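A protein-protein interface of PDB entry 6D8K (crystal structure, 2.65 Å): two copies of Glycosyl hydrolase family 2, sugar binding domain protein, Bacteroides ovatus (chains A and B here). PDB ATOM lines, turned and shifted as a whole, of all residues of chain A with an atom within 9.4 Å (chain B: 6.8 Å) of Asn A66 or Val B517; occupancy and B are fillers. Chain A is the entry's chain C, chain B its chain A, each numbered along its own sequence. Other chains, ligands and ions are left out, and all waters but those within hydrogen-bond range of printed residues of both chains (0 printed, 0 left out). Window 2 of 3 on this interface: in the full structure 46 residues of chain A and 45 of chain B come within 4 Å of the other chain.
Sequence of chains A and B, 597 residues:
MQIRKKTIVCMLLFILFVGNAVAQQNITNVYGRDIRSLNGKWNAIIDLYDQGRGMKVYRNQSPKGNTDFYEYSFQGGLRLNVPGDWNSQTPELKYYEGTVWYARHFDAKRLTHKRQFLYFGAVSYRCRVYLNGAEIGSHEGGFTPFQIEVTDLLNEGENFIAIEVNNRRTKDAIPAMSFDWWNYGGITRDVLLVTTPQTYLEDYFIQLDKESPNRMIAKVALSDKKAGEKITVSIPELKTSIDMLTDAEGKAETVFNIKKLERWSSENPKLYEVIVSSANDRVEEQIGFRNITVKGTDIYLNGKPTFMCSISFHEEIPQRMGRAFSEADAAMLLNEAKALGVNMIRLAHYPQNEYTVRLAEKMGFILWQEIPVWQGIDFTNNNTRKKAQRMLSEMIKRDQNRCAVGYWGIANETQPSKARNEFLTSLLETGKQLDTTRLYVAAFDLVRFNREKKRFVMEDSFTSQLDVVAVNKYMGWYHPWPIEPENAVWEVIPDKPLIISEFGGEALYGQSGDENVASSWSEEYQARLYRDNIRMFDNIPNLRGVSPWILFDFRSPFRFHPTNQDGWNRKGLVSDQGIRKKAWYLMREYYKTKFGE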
ATOM      1  N   SER A  62     -17.276 -14.235 -11.868  1.00  0.00           N
ATOM      2  CA  SER A  62     -18.517 -14.982 -11.801  1.00  0.00           C
ATOM      3  C   SER A  62     -18.341 -16.170 -10.864  1.00  0.00           C
ATOM      4  O   SER A  62     -17.229 -16.690 -10.729  1.00  0.00           O
ATOM      5  CB  SER A  62     -18.933 -15.490 -13.185  1.00  0.00           C
ATOM      6  OG  SER A  62     -19.779 -14.568 -13.843  1.00  0.00           O
ATOM      7  N   PRO A  63     -19.405 -16.608 -10.191  1.00  0.00           N
ATOM      8  CA  PRO A  63     -19.297 -17.787  -9.316  1.00  0.00           C
ATOM      9  C   PRO A  63     -18.888 -19.044 -10.082  1.00  0.00           C
ATOM     10  O   PRO A  63     -19.502 -19.418 -11.087  1.00  0.00           O
ATOM     11  CB  PRO A  63     -20.706 -17.914  -8.718  1.00  0.00           C
ATOM     12  CG  PRO A  63     -21.596 -17.053  -9.579  1.00  0.00           C
ATOM     13  CD  PRO A  63     -20.726 -15.961 -10.090  1.00  0.00           C
ATOM     14  N   LYS A  64     -17.843 -19.707  -9.578  1.00  0.00           N
ATOM     15  CA  LYS A  64     -17.262 -20.893 -10.199  1.00  0.00           C
ATOM     16  C   LYS A  64     -17.870 -22.192  -9.677  1.00  0.00           C
ATOM     17  O   LYS A  64     -18.141 -23.107 -10.465  1.00  0.00           O
ATOM     18  CB  LYS A  64     -15.742 -20.906  -9.979  1.00  0.00           C
ATOM     19  CG  LYS A  64     -14.911 -20.377 -11.168  1.00  0.00           C
ATOM     20  CD  LYS A  64     -15.093 -18.872 -11.406  1.00  0.00           C
ATOM     21  CE  LYS A  64     -14.561 -18.437 -12.791  1.00  0.00           C
ATOM     22  NZ  LYS A  64     -14.910 -17.023 -13.176  1.00  0.00           N
ATOM     23  N   GLY A  65     -18.107 -22.287  -8.370  1.00  0.00           N
ATOM     24  CA  GLY A  65     -18.544 -23.540  -7.790  1.00  0.00           C
ATOM     25  C   GLY A  65     -19.904 -23.517  -7.129  1.00  0.00           C
ATOM     26  O   GLY A  65     -20.898 -23.109  -7.739  1.00  0.00           O
ATOM     27  N   ASN A  66     -19.960 -23.991  -5.881  1.00  0.00           N
ATOM     28  CA  ASN A  66     -21.194 -24.078  -5.114  1.00  0.00           C
ATOM     29  C   ASN A  66     -21.126 -23.313  -3.793  1.00  0.00           C
ATOM     30  O   ASN A  66     -22.162 -23.133  -3.137  1.00  0.00           O
ATOM     31  CB  ASN A  66     -21.551 -25.554  -4.853  1.00  0.00           C
ATOM     32  CG  ASN A  66     -22.395 -26.180  -5.981  1.00  0.00           C
ATOM     33  OD1 ASN A  66     -22.515 -25.626  -7.072  1.00  0.00           O
ATOM     34  ND2 ASN A  66     -22.985 -27.338  -5.706  1.00  0.00           N
ATOM     35  N   THR A  67     -19.948 -22.827  -3.404  1.00  0.00           N
ATOM     36  CA  THR A  67     -19.793 -22.065  -2.181  1.00  0.00           C
ATOM     37  C   THR A  67     -19.404 -20.612  -2.405  1.00  0.00           C
ATOM     38  O   THR A  67     -19.488 -19.818  -1.459  1.00  0.00           O
ATOM     39  CB  THR A  67     -18.729 -22.713  -1.283  1.00  0.00           C
ATOM     40  OG1 THR A  67     -17.513 -22.864  -2.032  1.00  0.00           O
ATOM     41  CG2 THR A  67     -19.217 -24.062  -0.762  1.00  0.00           C
ATOM     42  N   ASP A  68     -18.959 -20.245  -3.602  1.00  0.00           N
ATOM     43  CA  ASP A  68     -18.464 -18.895  -3.836  1.00  0.00           C
ATOM     44  C   ASP A  68     -19.579 -18.003  -4.389  1.00  0.00           C
ATOM     45  O   ASP A  68     -20.530 -18.484  -5.012  1.00  0.00           O
ATOM     46  CB  ASP A  68     -17.257 -18.928  -4.782  1.00  0.00           C
ATOM     47  CG  ASP A  68     -17.589 -19.486  -6.157  1.00  0.00           C
ATOM     48  OD1 ASP A  68     -18.589 -20.221  -6.303  1.00  0.00           O
ATOM     49  OD2 ASP A  68     -16.826 -19.193  -7.106  1.00  0.00           O
ATOM     50  N   PHE A  69     -19.466 -16.695  -4.142  1.00  0.00           N
ATOM     51  CA  PHE A  69     -20.403 -15.751  -4.746  1.00  0.00           C
ATOM     52  C   PHE A  69     -19.817 -14.340  -4.766  1.00  0.00           C
ATOM     53  O   PHE A  69     -18.955 -13.983  -3.957  1.00  0.00           O
ATOM     54  CB  PHE A  69     -21.774 -15.781  -4.036  1.00  0.00           C
ATOM     55  CG  PHE A  69     -21.736 -15.388  -2.588  1.00  0.00           C
ATOM     56  CD1 PHE A  69     -21.869 -16.344  -1.601  1.00  0.00           C
ATOM     57  CD2 PHE A  69     -21.606 -14.059  -2.215  1.00  0.00           C
ATOM     58  CE1 PHE A  69     -21.840 -15.994  -0.273  1.00  0.00           C
ATOM     59  CE2 PHE A  69     -21.573 -13.693  -0.884  1.00  0.00           C
ATOM     60  CZ  PHE A  69     -21.688 -14.662   0.090  1.00  0.00           C
ATOM     61  N   GLY B 476     -21.892 -21.278   6.103  1.00  0.00           N
ATOM     62  CA  GLY B 476     -22.612 -21.538   4.875  1.00  0.00           C
ATOM     63  C   GLY B 476     -22.855 -20.324   3.998  1.00  0.00           C
ATOM     64  O   GLY B 476     -23.485 -20.459   2.939  1.00  0.00           O
ATOM     65  N   TRP B 477     -22.383 -19.144   4.400  1.00  0.00           N
ATOM     66  CA  TRP B 477     -22.544 -17.955   3.575  1.00  0.00           C
ATOM     67  C   TRP B 477     -21.196 -17.282   3.316  1.00  0.00           C
ATOM     68  O   TRP B 477     -20.540 -17.588   2.320  1.00  0.00           O
ATOM     69  CB  TRP B 477     -23.539 -16.978   4.225  1.00  0.00           C
ATOM     70  CG  TRP B 477     -23.878 -15.848   3.303  1.00  0.00           C
ATOM     71  CD1 TRP B 477     -23.605 -14.514   3.481  1.00  0.00           C
ATOM     72  CD2 TRP B 477     -24.494 -15.963   2.017  1.00  0.00           C
ATOM     73  NE1 TRP B 477     -24.037 -13.802   2.395  1.00  0.00           N
ATOM     74  CE2 TRP B 477     -24.589 -14.665   1.485  1.00  0.00           C
ATOM     75  CE3 TRP B 477     -24.987 -17.040   1.268  1.00  0.00           C
ATOM     76  CZ2 TRP B 477     -25.141 -14.418   0.242  1.00  0.00           C
ATOM     77  CZ3 TRP B 477     -25.547 -16.788   0.047  1.00  0.00           C
ATOM     78  CH2 TRP B 477     -25.613 -15.493  -0.460  1.00  0.00           C
ATOM     79  N   GLY B 513     -34.273 -21.727  -6.870  1.00  0.00           N
ATOM     80  CA  GLY B 513     -32.931 -22.090  -7.276  1.00  0.00           C
ATOM     81  C   GLY B 513     -32.472 -23.327  -6.543  1.00  0.00           C
ATOM     82  O   GLY B 513     -33.168 -23.868  -5.680  1.00  0.00           O
ATOM     83  N   ASP B 514     -31.272 -23.765  -6.895  1.00  0.00           N
ATOM     84  CA  ASP B 514     -30.780 -25.063  -6.456  1.00  0.00           C
ATOM     85  C   ASP B 514     -30.372 -24.980  -4.994  1.00  0.00           C
ATOM     86  O   ASP B 514     -29.492 -24.190  -4.635  1.00  0.00           O
ATOM     87  CB  ASP B 514     -29.611 -25.502  -7.340  1.00  0.00           C
ATOM     88  CG  ASP B 514     -29.295 -26.980  -7.200  1.00  0.00           C
ATOM     89  OD1 ASP B 514     -28.710 -27.361  -6.161  1.00  0.00           O
ATOM     90  OD2 ASP B 514     -29.645 -27.757  -8.119  1.00  0.00           O
ATOM     91  N   GLU B 515     -31.011 -25.811  -4.164  1.00  0.00           N
ATOM     92  CA  GLU B 515     -30.736 -25.932  -2.733  1.00  0.00           C
ATOM     93  C   GLU B 515     -29.248 -25.926  -2.381  1.00  0.00           C
ATOM     94  O   GLU B 515     -28.887 -25.525  -1.270  1.00  0.00           O
ATOM     95  CB  GLU B 515     -31.392 -27.225  -2.231  1.00  0.00           C
ATOM     96  CG  GLU B 515     -31.357 -27.469  -0.731  1.00  0.00           C
ATOM     97  CD  GLU B 515     -31.995 -28.803  -0.342  1.00  0.00           C
ATOM     98  OE1 GLU B 515     -31.321 -29.646   0.306  1.00  0.00           O
ATOM     99  OE2 GLU B 515     -33.179 -29.005  -0.692  1.00  0.00           O
ATOM    100  N   ASN B 516     -28.370 -26.348  -3.292  1.00  0.00           N
ATOM    101  CA  ASN B 516     -26.969 -26.549  -2.952  1.00  0.00           C
ATOM    102  C   ASN B 516     -26.035 -25.427  -3.394  1.00  0.00           C
ATOM    103  O   ASN B 516     -24.861 -25.450  -3.004  1.00  0.00           O
ATOM    104  CB  ASN B 516     -26.468 -27.880  -3.545  1.00  0.00           C
ATOM    105  CG  ASN B 516     -27.301 -29.087  -3.097  1.00  0.00           C
ATOM    106  OD1 ASN B 516     -27.252 -29.512  -1.934  1.00  0.00           O
ATOM    107  ND2 ASN B 516     -28.059 -29.650  -4.030  1.00  0.00           N
ATOM    108  N   VAL B 517     -26.515 -24.443  -4.165  1.00  0.00           N
ATOM    109  CA  VAL B 517     -25.670 -23.431  -4.807  1.00  0.00           C
ATOM    110  C   VAL B 517     -25.916 -22.086  -4.125  1.00  0.00           C
ATOM    111  O   VAL B 517     -26.997 -21.507  -4.266  1.00  0.00           O
ATOM    112  CB  VAL B 517     -25.957 -23.337  -6.315  1.00  0.00           C
ATOM    113  CG1 VAL B 517     -24.976 -22.396  -7.002  1.00  0.00           C
ATOM    114  CG2 VAL B 517     -25.953 -24.724  -6.981  1.00  0.00           C
ATOM    115  N   ALA B 518     -24.900 -21.553  -3.433  1.00  0.00           N
ATOM    116  CA  ALA B 518     -25.057 -20.300  -2.680  1.00  0.00           C
ATOM    117  C   ALA B 518     -25.374 -19.113  -3.588  1.00  0.00           C
ATOM    118  O   ALA B 518     -26.205 -18.262  -3.247  1.00  0.00           O
ATOM    119  CB  ALA B 518     -23.791 -20.002  -1.874  1.00  0.00           C
ATOM    120  N   SER B 519     -24.698 -19.021  -4.738  1.00  0.00           N
ATOM    121  CA  SER B 519     -24.932 -17.944  -5.678  1.00  0.00           C
ATOM    122  C   SER B 519     -26.282 -18.030  -6.337  1.00  0.00           C
ATOM    123  O   SER B 519     -26.606 -17.192  -7.202  1.00  0.00           O
ATOM    124  CB  SER B 519     -23.830 -17.934  -6.738  1.00  0.00           C
ATOM    125  OG  SER B 519     -23.896 -19.095  -7.548  1.00  0.00           O
ATOM    126  N   SER B 520     -27.142 -18.995  -6.011  1.00  0.00           N
ATOM    127  CA  SER B 520     -28.451 -19.015  -6.647  1.00  0.00           C
ATOM    128  C   SER B 520     -29.345 -17.871  -6.168  1.00  0.00           C
ATOM    129  O   SER B 520     -30.328 -17.547  -6.848  1.00  0.00           O
ATOM    130  CB  SER B 520     -29.151 -20.349  -6.386  1.00  0.00           C
ATOM    131  OG  SER B 520     -29.463 -20.502  -5.013  1.00  0.00           O
ATOM    132  N   TRP B 521     -29.026 -17.266  -5.014  1.00  0.00           N
ATOM    133  CA  TRP B 521     -29.901 -16.288  -4.359  1.00  0.00           C
ATOM    134  C   TRP B 521     -31.326 -16.816  -4.277  1.00  0.00           C
ATOM    135  O   TRP B 521     -32.299 -16.074  -4.427  1.00  0.00           O
ATOM    136  CB  TRP B 521     -29.872 -14.927  -5.073  1.00  0.00           C
ATOM    137  CG  TRP B 521     -29.102 -13.859  -4.331  1.00  0.00           C
ATOM    138  CD1 TRP B 521     -29.611 -12.927  -3.468  1.00  0.00           C
ATOM    139  CD2 TRP B 521     -27.693 -13.618  -4.389  1.00  0.00           C
ATOM    140  NE1 TRP B 521     -28.605 -12.128  -2.982  1.00  0.00           N
ATOM    141  CE2 TRP B 521     -27.416 -12.529  -3.525  1.00  0.00           C
ATOM    142  CE3 TRP B 521     -26.632 -14.228  -5.074  1.00  0.00           C
ATOM    143  CZ2 TRP B 521     -26.128 -12.036  -3.328  1.00  0.00           C
ATOM    144  CZ3 TRP B 521     -25.353 -13.737  -4.884  1.00  0.00           C
ATOM    145  CH2 TRP B 521     -25.112 -12.642  -4.022  1.00  0.00           C
ATOM    146  N   SER B 522     -31.454 -18.120  -4.091  1.00  0.00           N
ATOM    147  CA  SER B 522     -32.749 -18.763  -4.018  1.00  0.00           C
ATOM    148  C   SER B 522     -33.219 -18.798  -2.576  1.00  0.00           C
ATOM    149  O   SER B 522     -32.415 -18.902  -1.644  1.00  0.00           O
ATOM    150  CB  SER B 522     -32.674 -20.185  -4.567  1.00  0.00           C
ATOM    151  OG  SER B 522     -31.691 -20.951  -3.897  1.00  0.00           O
ATOM    152  N   TYR B 525     -31.919 -22.161  -1.189  1.00  0.00           N
ATOM    153  CA  TYR B 525     -30.605 -22.194  -0.550  1.00  0.00           C
ATOM    154  C   TYR B 525     -30.659 -21.579   0.848  1.00  0.00           C
ATOM    155  O   TYR B 525     -30.086 -22.129   1.794  1.00  0.00           O
ATOM    156  CB  TYR B 525     -29.536 -21.507  -1.415  1.00  0.00           C
ATOM    157  CG  TYR B 525     -28.150 -21.614  -0.790  1.00  0.00           C
ATOM    158  CD1 TYR B 525     -27.270 -22.630  -1.153  1.00  0.00           C
ATOM    159  CD2 TYR B 525     -27.744 -20.726   0.205  1.00  0.00           C
ATOM    160  CE1 TYR B 525     -26.018 -22.743  -0.553  1.00  0.00           C
ATOM    161  CE2 TYR B 525     -26.504 -20.832   0.804  1.00  0.00           C
ATOM    162  CZ  TYR B 525     -25.639 -21.841   0.425  1.00  0.00           C
ATOM    163  OH  TYR B 525     -24.403 -21.929   1.027  1.00  0.00           O
ATOM    164  N   ARG B 528     -32.071 -24.043   3.492  1.00  0.00           N
ATOM    165  CA  ARG B 528     -31.103 -25.082   3.850  1.00  0.00           C
ATOM    166  C   ARG B 528     -29.992 -24.537   4.738  1.00  0.00           C
ATOM    167  O   ARG B 528     -29.635 -25.159   5.751  1.00  0.00           O
ATOM    168  CB  ARG B 528     -30.503 -25.704   2.589  1.00  0.00           C
ATOM    169  CG  ARG B 528     -29.207 -26.457   2.852  1.00  0.00           C
ATOM    170  CD  ARG B 528     -28.221 -26.288   1.707  1.00  0.00           C
ATOM    171  NE  ARG B 528     -26.906 -26.840   2.039  1.00  0.00           N
ATOM    172  CZ  ARG B 528     -26.480 -28.031   1.634  1.00  0.00           C
ATOM    173  NH1 ARG B 528     -27.261 -28.793   0.882  1.00  0.00           N
ATOM    174  NH2 ARG B 528     -25.277 -28.462   1.977  1.00  0.00           N
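The backbone carbonyl oxygen of Asn A66 is in hydrogen-bond range of the backbone NH of Ala B518 (3.2 Å).
O of Val B517 sits at hydrogen-bond distance from OG of Ser B520 (2.8 Å).
The side-chain carboxylate (OD1) of Asp B514 sits close to the backbone NH (N) of Asn B516 (3.1 Å).
The guanidinium group (NH1) of Arg B528 is in hydrogen-bond range of the side-chain amide oxygen (OD1) of Asn B516 (2.9 Å).
The backbone NH (N) of Lys A64 is in hydrogen-bond range of the side-chain carboxylate (OD2) of Asp A68, 2.7 Å away.
The side-chain carboxylate of Asp A68 is in hydrogen-bond range of the backbone NH of Gly A65.
Among the printed residues, merely in contact across the chains: Pro A63 with Ser B519 (3.6 Å), Asn A66 with Asn B516 (3.6 Å), Asn A66 with Val B517 (3.6 Å), Asp A68 with Ser B519 (3.8 Å) and Phe A69 with Trp B477 (3.2 Å).
Asn A66 touches just these residues of chain B: Asn B516, Val B517 and Ala B518.
Of the printed residues of chain B, Asp A68 touches Ser B519 (3.8 Å).
Printed residues of chain A within 4 Å of Trp B477: Phe A69 (3.2 Å).
Gly B513 touches none of the printed residues of chain A.
Val B517 touches just one residue of chain A: Asn A66.
Ala B518 touches just one residue of chain A: Asn A66 (3.2 Å).
Ser B519 touches just these residues of chain A: Pro A63 (3.6 Å) and Asp A68 (3.8 Å).
The nearest residue of chain B that does not touch Asn A66 is Tyr B525 (4.7 Å).
The nearest residue of chain A that does not touch Val B517 is Gly A65 (4.2 Å).
The nearest printed residue of chain B that does not touch Phe A69 is Ser B519 (4.02 Å).
Of the 14 printed residues of chain B, 5 touch a printed residue of chain A.
Hydrophobic or aromatic side chains of chain B within 4 Å of the printed part of chain A: Trp B477, Val B517 and Ala B518.
Among the printed residues, no Asp or Glu carboxylate lies within 4 Å of a Lys or Arg side-chain nitrogen of the other chain.
No position is printed for both chains.
Of the 6 pairs that touch across the chains among the printed residues, none has its exchanged pair printed and touching as well.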
